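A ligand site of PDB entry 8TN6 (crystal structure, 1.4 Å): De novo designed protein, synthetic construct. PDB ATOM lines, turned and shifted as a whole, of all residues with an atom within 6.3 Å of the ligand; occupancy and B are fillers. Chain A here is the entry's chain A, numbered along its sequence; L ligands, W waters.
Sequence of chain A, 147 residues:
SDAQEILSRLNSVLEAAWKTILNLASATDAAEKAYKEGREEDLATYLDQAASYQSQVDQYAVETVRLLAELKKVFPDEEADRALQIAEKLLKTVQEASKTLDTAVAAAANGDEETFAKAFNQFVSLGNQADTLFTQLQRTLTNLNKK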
ATOM      1  N   TRP A  18     -20.606  -8.386   9.328  1.00  0.00           N
ATOM      2  CA  TRP A  18     -19.986  -7.383   8.473  1.00  0.00           C
ATOM      3  C   TRP A  18     -18.499  -7.231   8.782  1.00  0.00           C
ATOM      4  O   TRP A  18     -17.692  -7.058   7.871  1.00  0.00           O
ATOM      5  CB  TRP A  18     -20.696  -6.037   8.565  1.00  0.00           C
ATOM      6  CG  TRP A  18     -20.137  -5.098   7.543  1.00  0.00           C
ATOM      7  CD1 TRP A  18     -19.390  -3.979   7.779  1.00  0.00           C
ATOM      8  CD2 TRP A  18     -20.227  -5.235   6.121  1.00  0.00           C
ATOM      9  NE1 TRP A  18     -19.041  -3.379   6.582  1.00  0.00           N
ATOM     10  CE2 TRP A  18     -19.531  -4.139   5.546  1.00  0.00           C
ATOM     11  CE3 TRP A  18     -20.833  -6.164   5.272  1.00  0.00           C
ATOM     12  CZ2 TRP A  18     -19.435  -3.957   4.166  1.00  0.00           C
ATOM     13  CZ3 TRP A  18     -20.732  -5.973   3.893  1.00  0.00           C
ATOM     14  CH2 TRP A  18     -20.041  -4.878   3.360  1.00  0.00           C
ATOM     15  N   ILE A  21     -16.853 -10.148   7.097  1.00  0.00           N
ATOM     16  CA  ILE A  21     -16.829  -9.910   5.650  1.00  0.00           C
ATOM     17  C   ILE A  21     -15.665  -8.975   5.298  1.00  0.00           C
ATOM     18  O   ILE A  21     -14.922  -9.230   4.350  1.00  0.00           O
ATOM     19  CB  ILE A  21     -18.191  -9.377   5.157  1.00  0.00           C
ATOM     20  CG1 ILE A  21     -19.197 -10.519   5.121  1.00  0.00           C
ATOM     21  CG2 ILE A  21     -18.052  -8.739   3.800  1.00  0.00           C
ATOM     22  CD1 ILE A  21     -20.616 -10.042   5.142  1.00  0.00           C
ATOM     23  N   LEU A  24     -12.644 -10.976   5.463  1.00  0.00           N
ATOM     24  CA  LEU A  24     -12.601 -11.876   4.324  1.00  0.00           C
ATOM     25  C   LEU A  24     -12.138 -11.130   3.078  1.00  0.00           C
ATOM     26  O   LEU A  24     -11.308 -11.633   2.320  1.00  0.00           O
ATOM     27  CB  LEU A  24     -13.976 -12.504   4.108  1.00  0.00           C
ATOM     28  CG  LEU A  24     -14.172 -13.442   2.932  1.00  0.00           C
ATOM     29  CD1 LEU A  24     -13.165 -14.539   2.944  1.00  0.00           C
ATOM     30  CD2 LEU A  24     -15.583 -13.998   2.993  1.00  0.00           C
ATOM     31  N   ALA A  25     -12.651  -9.918   2.871  1.00  0.00           N
ATOM     32  CA  ALA A  25     -12.237  -9.159   1.713  1.00  0.00           C
ATOM     33  C   ALA A  25     -10.751  -8.848   1.762  1.00  0.00           C
ATOM     34  O   ALA A  25     -10.090  -8.929   0.724  1.00  0.00           O
ATOM     35  CB  ALA A  25     -13.032  -7.871   1.621  1.00  0.00           C
ATOM     36  N   SER A  26     -10.208  -8.514   2.933  1.00  0.00           N
ATOM     37  CA  SER A  26      -8.783  -8.214   3.026  1.00  0.00           C
ATOM     38  C   SER A  26      -7.948  -9.442   2.708  1.00  0.00           C
ATOM     39  O   SER A  26      -6.907  -9.333   2.053  1.00  0.00           O
ATOM     40  CB  SER A  26      -8.385  -7.600   4.372  1.00  0.00           C
ATOM     41  OG  SER A  26      -8.536  -8.508   5.447  1.00  0.00           O
ATOM     42  N   THR A  28      -8.867 -11.974   0.828  1.00  0.00           N
ATOM     43  CA  THR A  28      -9.046 -12.244  -0.587  1.00  0.00           C
ATOM     44  C   THR A  28      -8.160 -11.342  -1.417  1.00  0.00           C
ATOM     45  O   THR A  28      -7.516 -11.795  -2.377  1.00  0.00           O
ATOM     46  CB  THR A  28     -10.523 -12.047  -0.936  1.00  0.00           C
ATOM     47  OG1 THR A  28     -11.338 -12.967  -0.185  1.00  0.00           O
ATOM     48  CG2 THR A  28     -10.798 -12.283  -2.399  1.00  0.00           C
ATOM     49  N   ASP A  29      -8.104 -10.059  -1.091  1.00  0.00           N
ATOM     50  CA  ASP A  29      -7.268  -9.130  -1.823  1.00  0.00           C
ATOM     51  C   ASP A  29      -5.799  -9.441  -1.641  1.00  0.00           C
ATOM     52  O   ASP A  29      -5.020  -9.366  -2.605  1.00  0.00           O
ATOM     53  CB  ASP A  29      -7.628  -7.715  -1.394  1.00  0.00           C
ATOM     54  CG  ASP A  29      -9.022  -7.317  -1.893  1.00  0.00           C
ATOM     55  OD1 ASP A  29      -9.665  -8.135  -2.621  1.00  0.00           O
ATOM     56  OD2 ASP A  29      -9.506  -6.240  -1.503  1.00  0.00           O
ATOM     57  N   GLN A  54     -14.626 -17.374   5.655  1.00  0.00           N
ATOM     58  CA  GLN A  54     -15.811 -17.781   4.920  1.00  0.00           C
ATOM     59  C   GLN A  54     -16.676 -18.722   5.743  1.00  0.00           C
ATOM     60  O   GLN A  54     -17.901 -18.619   5.724  1.00  0.00           O
ATOM     61  CB  GLN A  54     -15.384 -18.469   3.629  1.00  0.00           C
ATOM     62  CG  GLN A  54     -16.534 -18.901   2.775  1.00  0.00           C
ATOM     63  CD  GLN A  54     -17.280 -17.737   2.195  1.00  0.00           C
ATOM     64  OE1 GLN A  54     -16.747 -17.018   1.376  1.00  0.00           O
ATOM     65  NE2 GLN A  54     -18.482 -17.474   2.664  1.00  0.00           N
ATOM     66  N   VAL A  57     -18.652 -16.583   8.040  1.00  0.00           N
ATOM     67  CA  VAL A  57     -19.732 -15.874   7.368  1.00  0.00           C
ATOM     68  C   VAL A  57     -20.893 -16.831   7.138  1.00  0.00           C
ATOM     69  O   VAL A  57     -22.048 -16.470   7.364  1.00  0.00           O
ATOM     70  CB  VAL A  57     -19.267 -15.245   6.034  1.00  0.00           C
ATOM     71  CG1 VAL A  57     -20.431 -14.642   5.293  1.00  0.00           C
ATOM     72  CG2 VAL A  57     -18.164 -14.202   6.302  1.00  0.00           C
ATOM     73  N   ASP A  58     -20.582 -18.038   6.672  1.00  0.00           N
ATOM     74  CA  ASP A  58     -21.612 -19.037   6.446  1.00  0.00           C
ATOM     75  C   ASP A  58     -22.407 -19.288   7.719  1.00  0.00           C
ATOM     76  O   ASP A  58     -23.642 -19.323   7.691  1.00  0.00           O
ATOM     77  CB  ASP A  58     -20.990 -20.335   5.952  1.00  0.00           C
ATOM     78  CG  ASP A  58     -20.460 -20.242   4.545  1.00  0.00           C
ATOM     79  OD1 ASP A  58     -19.946 -21.271   4.069  1.00  0.00           O
ATOM     80  OD2 ASP A  58     -20.575 -19.170   3.951  1.00  0.00           O
ATOM     81  N   LEU A  90     -29.310 -14.571   0.619  1.00  0.00           N
ATOM     82  CA  LEU A  90     -27.963 -14.289   1.100  1.00  0.00           C
ATOM     83  C   LEU A  90     -27.246 -15.575   1.493  1.00  0.00           C
ATOM     84  O   LEU A  90     -26.086 -15.781   1.127  1.00  0.00           O
ATOM     85  CB  LEU A  90     -28.005 -13.346   2.286  1.00  0.00           C
ATOM     86  CG  LEU A  90     -26.695 -12.997   2.983  1.00  0.00           C
ATOM     87  CD1 LEU A  90     -25.729 -12.285   2.027  1.00  0.00           C
ATOM     88  CD2 LEU A  90     -26.959 -12.134   4.185  1.00  0.00           C
ATOM     89  N   THR A  93     -26.175 -17.494  -1.439  1.00  0.00           N
ATOM     90  CA  THR A  93     -25.069 -16.875  -2.157  1.00  0.00           C
ATOM     91  C   THR A  93     -23.768 -17.109  -1.423  1.00  0.00           C
ATOM     92  O   THR A  93     -22.754 -17.446  -2.050  1.00  0.00           O
ATOM     93  CB  THR A  93     -25.358 -15.402  -2.364  1.00  0.00           C
ATOM     94  OG1 THR A  93     -26.606 -15.283  -3.047  1.00  0.00           O
ATOM     95  CG2 THR A  93     -24.301 -14.788  -3.199  1.00  0.00           C
ATOM     96  N   VAL A  94     -23.770 -16.962  -0.083  1.00  0.00           N
ATOM     97  CA  VAL A  94     -22.543 -17.182   0.658  1.00  0.00           C
ATOM     98  C   VAL A  94     -22.135 -18.638   0.584  1.00  0.00           C
ATOM     99  O   VAL A  94     -20.945 -18.945   0.556  1.00  0.00           O
ATOM    100  CB  VAL A  94     -22.567 -16.639   2.089  1.00  0.00           C
ATOM    101  CG1 VAL A  94     -22.988 -15.205   2.110  1.00  0.00           C
ATOM    102  CG2 VAL A  94     -23.395 -17.417   2.983  1.00  0.00           C
ATOM    103  N   ALA A  97     -20.437 -19.026  -2.639  1.00  0.00           N
ATOM    104  CA  ALA A  97     -19.084 -18.487  -2.486  1.00  0.00           C
ATOM    105  C   ALA A  97     -18.189 -19.498  -1.783  1.00  0.00           C
ATOM    106  O   ALA A  97     -17.050 -19.711  -2.179  1.00  0.00           O
ATOM    107  CB  ALA A  97     -19.128 -17.163  -1.720  1.00  0.00           C
ATOM    108  N   SER A  98     -18.689 -20.139  -0.732  1.00  0.00           N
ATOM    109  CA  SER A  98     -17.900 -21.115  -0.006  1.00  0.00           C
ATOM    110  C   SER A  98     -17.490 -22.278  -0.899  1.00  0.00           C
ATOM    111  O   SER A  98     -16.338 -22.736  -0.845  1.00  0.00           O
ATOM    112  CB  SER A  98     -18.710 -21.604   1.194  1.00  0.00           C
ATOM    113  OG  SER A  98     -17.851 -22.210   2.141  1.00  0.00           O
ATOM    114  N   PHE A 123     -15.358 -16.290  -7.165  1.00  0.00           N
ATOM    115  CA  PHE A 123     -15.529 -16.036  -5.735  1.00  0.00           C
ATOM    116  C   PHE A 123     -15.778 -14.562  -5.458  1.00  0.00           C
ATOM    117  O   PHE A 123     -16.686 -14.186  -4.723  1.00  0.00           O
ATOM    118  CB  PHE A 123     -14.290 -16.542  -5.016  1.00  0.00           C
ATOM    119  CG  PHE A 123     -14.325 -16.338  -3.524  1.00  0.00           C
ATOM    120  CD1 PHE A 123     -15.194 -17.041  -2.736  1.00  0.00           C
ATOM    121  CD2 PHE A 123     -13.511 -15.394  -2.933  1.00  0.00           C
ATOM    122  CE1 PHE A 123     -15.216 -16.824  -1.354  1.00  0.00           C
ATOM    123  CE2 PHE A 123     -13.528 -15.205  -1.555  1.00  0.00           C
ATOM    124  CZ  PHE A 123     -14.396 -15.919  -0.790  1.00  0.00           C
ATOM    125  N   VAL A 124     -14.976 -13.693  -6.084  1.00  0.00           N
ATOM    126  CA  VAL A 124     -15.150 -12.262  -5.901  1.00  0.00           C
ATOM    127  C   VAL A 124     -16.502 -11.791  -6.444  1.00  0.00           C
ATOM    128  O   VAL A 124     -17.193 -10.969  -5.832  1.00  0.00           O
ATOM    129  CB  VAL A 124     -13.965 -11.510  -6.534  1.00  0.00           C
ATOM    130  CG1 VAL A 124     -14.220 -10.016  -6.568  1.00  0.00           C
ATOM    131  CG2 VAL A 124     -12.695 -11.835  -5.771  1.00  0.00           C
ATOM    132  N   LEU A 126     -19.285 -13.485  -6.633  1.00  0.00           N
ATOM    133  CA  LEU A 126     -20.296 -13.888  -5.658  1.00  0.00           C
ATOM    134  C   LEU A 126     -20.247 -12.999  -4.436  1.00  0.00           C
ATOM    135  O   LEU A 126     -21.292 -12.699  -3.843  1.00  0.00           O
ATOM    136  CB  LEU A 126     -20.082 -15.348  -5.301  1.00  0.00           C
ATOM    137  CG  LEU A 126     -20.488 -16.305  -6.423  1.00  0.00           C
ATOM    138  CD1 LEU A 126     -19.860 -17.670  -6.228  1.00  0.00           C
ATOM    139  CD2 LEU A 126     -22.010 -16.414  -6.551  1.00  0.00           C
ATOM    140  N   GLY A 127     -19.050 -12.557  -4.041  1.00  0.00           N
ATOM    141  CA  GLY A 127     -18.957 -11.627  -2.929  1.00  0.00           C
ATOM    142  C   GLY A 127     -19.665 -10.311  -3.186  1.00  0.00           C
ATOM    143  O   GLY A 127     -20.347  -9.762  -2.321  1.00  0.00           O
ATOM    144  N   ASN A 128     -19.535  -9.777  -4.406  1.00  0.00           N
ATOM    145  CA  ASN A 128     -20.223  -8.534  -4.685  1.00  0.00           C
ATOM    146  C   ASN A 128     -21.734  -8.744  -4.717  1.00  0.00           C
ATOM    147  O   ASN A 128     -22.489  -7.889  -4.247  1.00  0.00           O
ATOM    148  CB  ASN A 128     -19.663  -7.891  -5.954  1.00  0.00           C
ATOM    149  CG  ASN A 128     -18.284  -7.315  -5.726  1.00  0.00           C
ATOM    150  OD1 ASN A 128     -17.374  -7.567  -6.504  1.00  0.00           O
ATOM    151  ND2 ASN A 128     -18.141  -6.538  -4.650  1.00  0.00           N
ATOM    152  N   ALA A 130     -23.299 -11.041  -2.841  1.00  0.00           N
ATOM    153  CA  ALA A 130     -23.691 -11.178  -1.451  1.00  0.00           C
ATOM    154  C   ALA A 130     -23.739  -9.818  -0.771  1.00  0.00           C
ATOM    155  O   ALA A 130     -24.637  -9.552   0.019  1.00  0.00           O
ATOM    156  CB  ALA A 130     -22.751 -12.114  -0.710  1.00  0.00           C
ATOM    157  N   ASP A 131     -22.788  -8.935  -1.092  1.00  0.00           N
ATOM    158  CA  ASP A 131     -22.793  -7.597  -0.500  1.00  0.00           C
ATOM    159  C   ASP A 131     -24.097  -6.865  -0.805  1.00  0.00           C
ATOM    160  O   ASP A 131     -24.688  -6.221   0.076  1.00  0.00           O
ATOM    161  CB  ASP A 131     -21.568  -6.834  -1.023  1.00  0.00           C
ATOM    162  CG  ASP A 131     -21.503  -5.401  -0.534  1.00  0.00           C
ATOM    163  OD1 ASP A 131     -22.350  -4.562  -0.931  1.00  0.00           O
ATOM    164  OD2 ASP A 131     -20.561  -5.110   0.234  1.00  0.00           O
ATOM    165  N   PHE A 134     -26.726  -8.310   1.382  1.00  0.00           N
ATOM    166  CA  PHE A 134     -26.506  -7.957   2.785  1.00  0.00           C
ATOM    167  C   PHE A 134     -27.017  -6.545   3.064  1.00  0.00           C
ATOM    168  O   PHE A 134     -27.687  -6.286   4.068  1.00  0.00           O
ATOM    169  CB  PHE A 134     -25.015  -8.061   3.067  1.00  0.00           C
ATOM    170  CG  PHE A 134     -24.658  -8.026   4.523  1.00  0.00           C
ATOM    171  CD1 PHE A 134     -24.609  -6.832   5.212  1.00  0.00           C
ATOM    172  CD2 PHE A 134     -24.353  -9.200   5.199  1.00  0.00           C
ATOM    173  CE1 PHE A 134     -24.276  -6.809   6.578  1.00  0.00           C
ATOM    174  CE2 PHE A 134     -24.027  -9.182   6.544  1.00  0.00           C
ATOM    175  CZ  PHE A 134     -23.993  -7.990   7.223  1.00  0.00           C
HETATM  176  O1  LIG L   1     -19.271 -14.654   2.147  1.00  0.00           O
HETATM  177  C1  LIG L   1     -18.817 -13.921   1.245  1.00  0.00           C
HETATM  178  N1  LIG L   1     -17.918 -14.512   0.387  1.00  0.00           N
HETATM  179  C2  LIG L   1     -17.383 -14.081  -0.627  1.00  0.00           C
HETATM  180  C3  LIG L   1     -16.118 -13.017  -0.490  1.00  0.00           C
HETATM  181  C4  LIG L   1     -17.105 -11.515  -0.150  1.00  0.00           C
HETATM  182  C5  LIG L   1     -18.507 -11.768   0.665  1.00  0.00           C
HETATM  183  C6  LIG L   1     -19.151 -12.772   1.187  1.00  0.00           C
HETATM  184  C7  LIG L   1     -20.419 -12.346   1.827  1.00  0.00           C
HETATM  185  C8  LIG L   1     -20.808 -10.979   1.796  1.00  0.00           C
HETATM  186  F1  LIG L   1     -22.009 -10.693   2.390  1.00  0.00           F
HETATM  187  C9  LIG L   1     -20.099 -10.026   1.220  1.00  0.00           C
HETATM  188  C10 LIG L   1     -18.999 -10.344   0.660  1.00  0.00           C
HETATM  189  N2  LIG L   1     -18.012  -9.624  -0.003  1.00  0.00           N
HETATM  190  C11 LIG L   1     -17.019 -10.281  -0.432  1.00  0.00           C
HETATM  191  C12 LIG L   1     -15.852  -9.708  -1.242  1.00  0.00           C
HETATM  192  C13 LIG L   1     -16.200  -8.705  -2.122  1.00  0.00           C
HETATM  193  C14 LIG L   1     -15.224  -8.158  -2.951  1.00  0.00           C
HETATM  194  C15 LIG L   1     -14.531 -10.158  -1.221  1.00  0.00           C
HETATM  195  C16 LIG L   1     -13.551  -9.588  -2.047  1.00  0.00           C
HETATM  196  C17 LIG L   1     -13.907  -8.580  -2.925  1.00  0.00           C
HETATM  197  C18 LIG L   1     -12.823  -7.977  -3.836  1.00  0.00           C
HETATM  198  N3  LIG L   1     -12.338  -6.719  -3.274  1.00  0.00           N
HETATM  199  C19 LIG L   1     -11.584  -5.965  -4.278  1.00  0.00           C
HETATM  200  O   HOH W   1     -17.951  -6.557   0.239  1.00  0.00           O
HETATM  201  O   HOH W   2     -16.793  -5.338  -1.965  1.00  0.00           O
HETATM  202  O   HOH W   3     -13.944  -4.976  -1.704  1.00  0.00           O
HETATM  203  O   HOH W   4     -14.823  -6.303  -5.995  1.00  0.00           O
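A nitrogen (N1) of the ligand is in hydrogen-bond range of the side-chain amide oxygen of Gln 54, at 2.9 Å. The side-chain carboxylate (OD1) of Asp 29 is in salt-bridge range of a nitrogen (N3) of the ligand, at 3.1 Å. O of Gly 127 is in hydrogen-bond range of N2 of the ligand (3.3 Å).
The side-chain carboxylate (OD2) of Asp 58 is in hydrogen-bond range of the side-chain amide nitrogen (NE2) of Gln 54 (3.0 Å). The backbone carbonyl oxygen (O) of Val 124 lies close to the side-chain amide oxygen (OD1) of Asn 128 (3.5 Å). OG1 of Thr 28 sits at hydrogen-bond distance from O of Leu 24.
Ile 21 touches the ligand. Leu 24 touches the ligand (CD2 to N1, 3.5 Å). CA of Ala 25 touches C15 of the ligand, at 3.9 Å. Thr 28 touches the ligand. Val 57 touches the ligand. CG1 of Val 94 touches O1 of the ligand (3.8 Å). Ala 97 touches the ligand (CB to N1, 3.6 Å). Phe 123 touches the ligand. CG1 of Val 124 touches C18 of the ligand (3.7 Å). Asn 128 touches the ligand. Ala 130 touches the ligand (CB to C8, 3.4 Å). Asp 131 touches the ligand (N to C9, 3.7 Å). CD2 of Phe 134 touches F1 of the ligand, at 3.95 Å. 16 residues have an atom within 4 Å of the ligand: Ile 21, Leu 24, Ala 25, Thr 28, Asp 29, Gln 54, Val 57, Val 94, Ala 97, Phe 123, Val 124, Gly 127, Asn 128, Ala 130, Asp 131 and Phe 134.
Water W1 lies within hydrogen-bond range of OD2 of Asp 131 (3.0 Å) and N2 of the ligand (3.1 Å).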
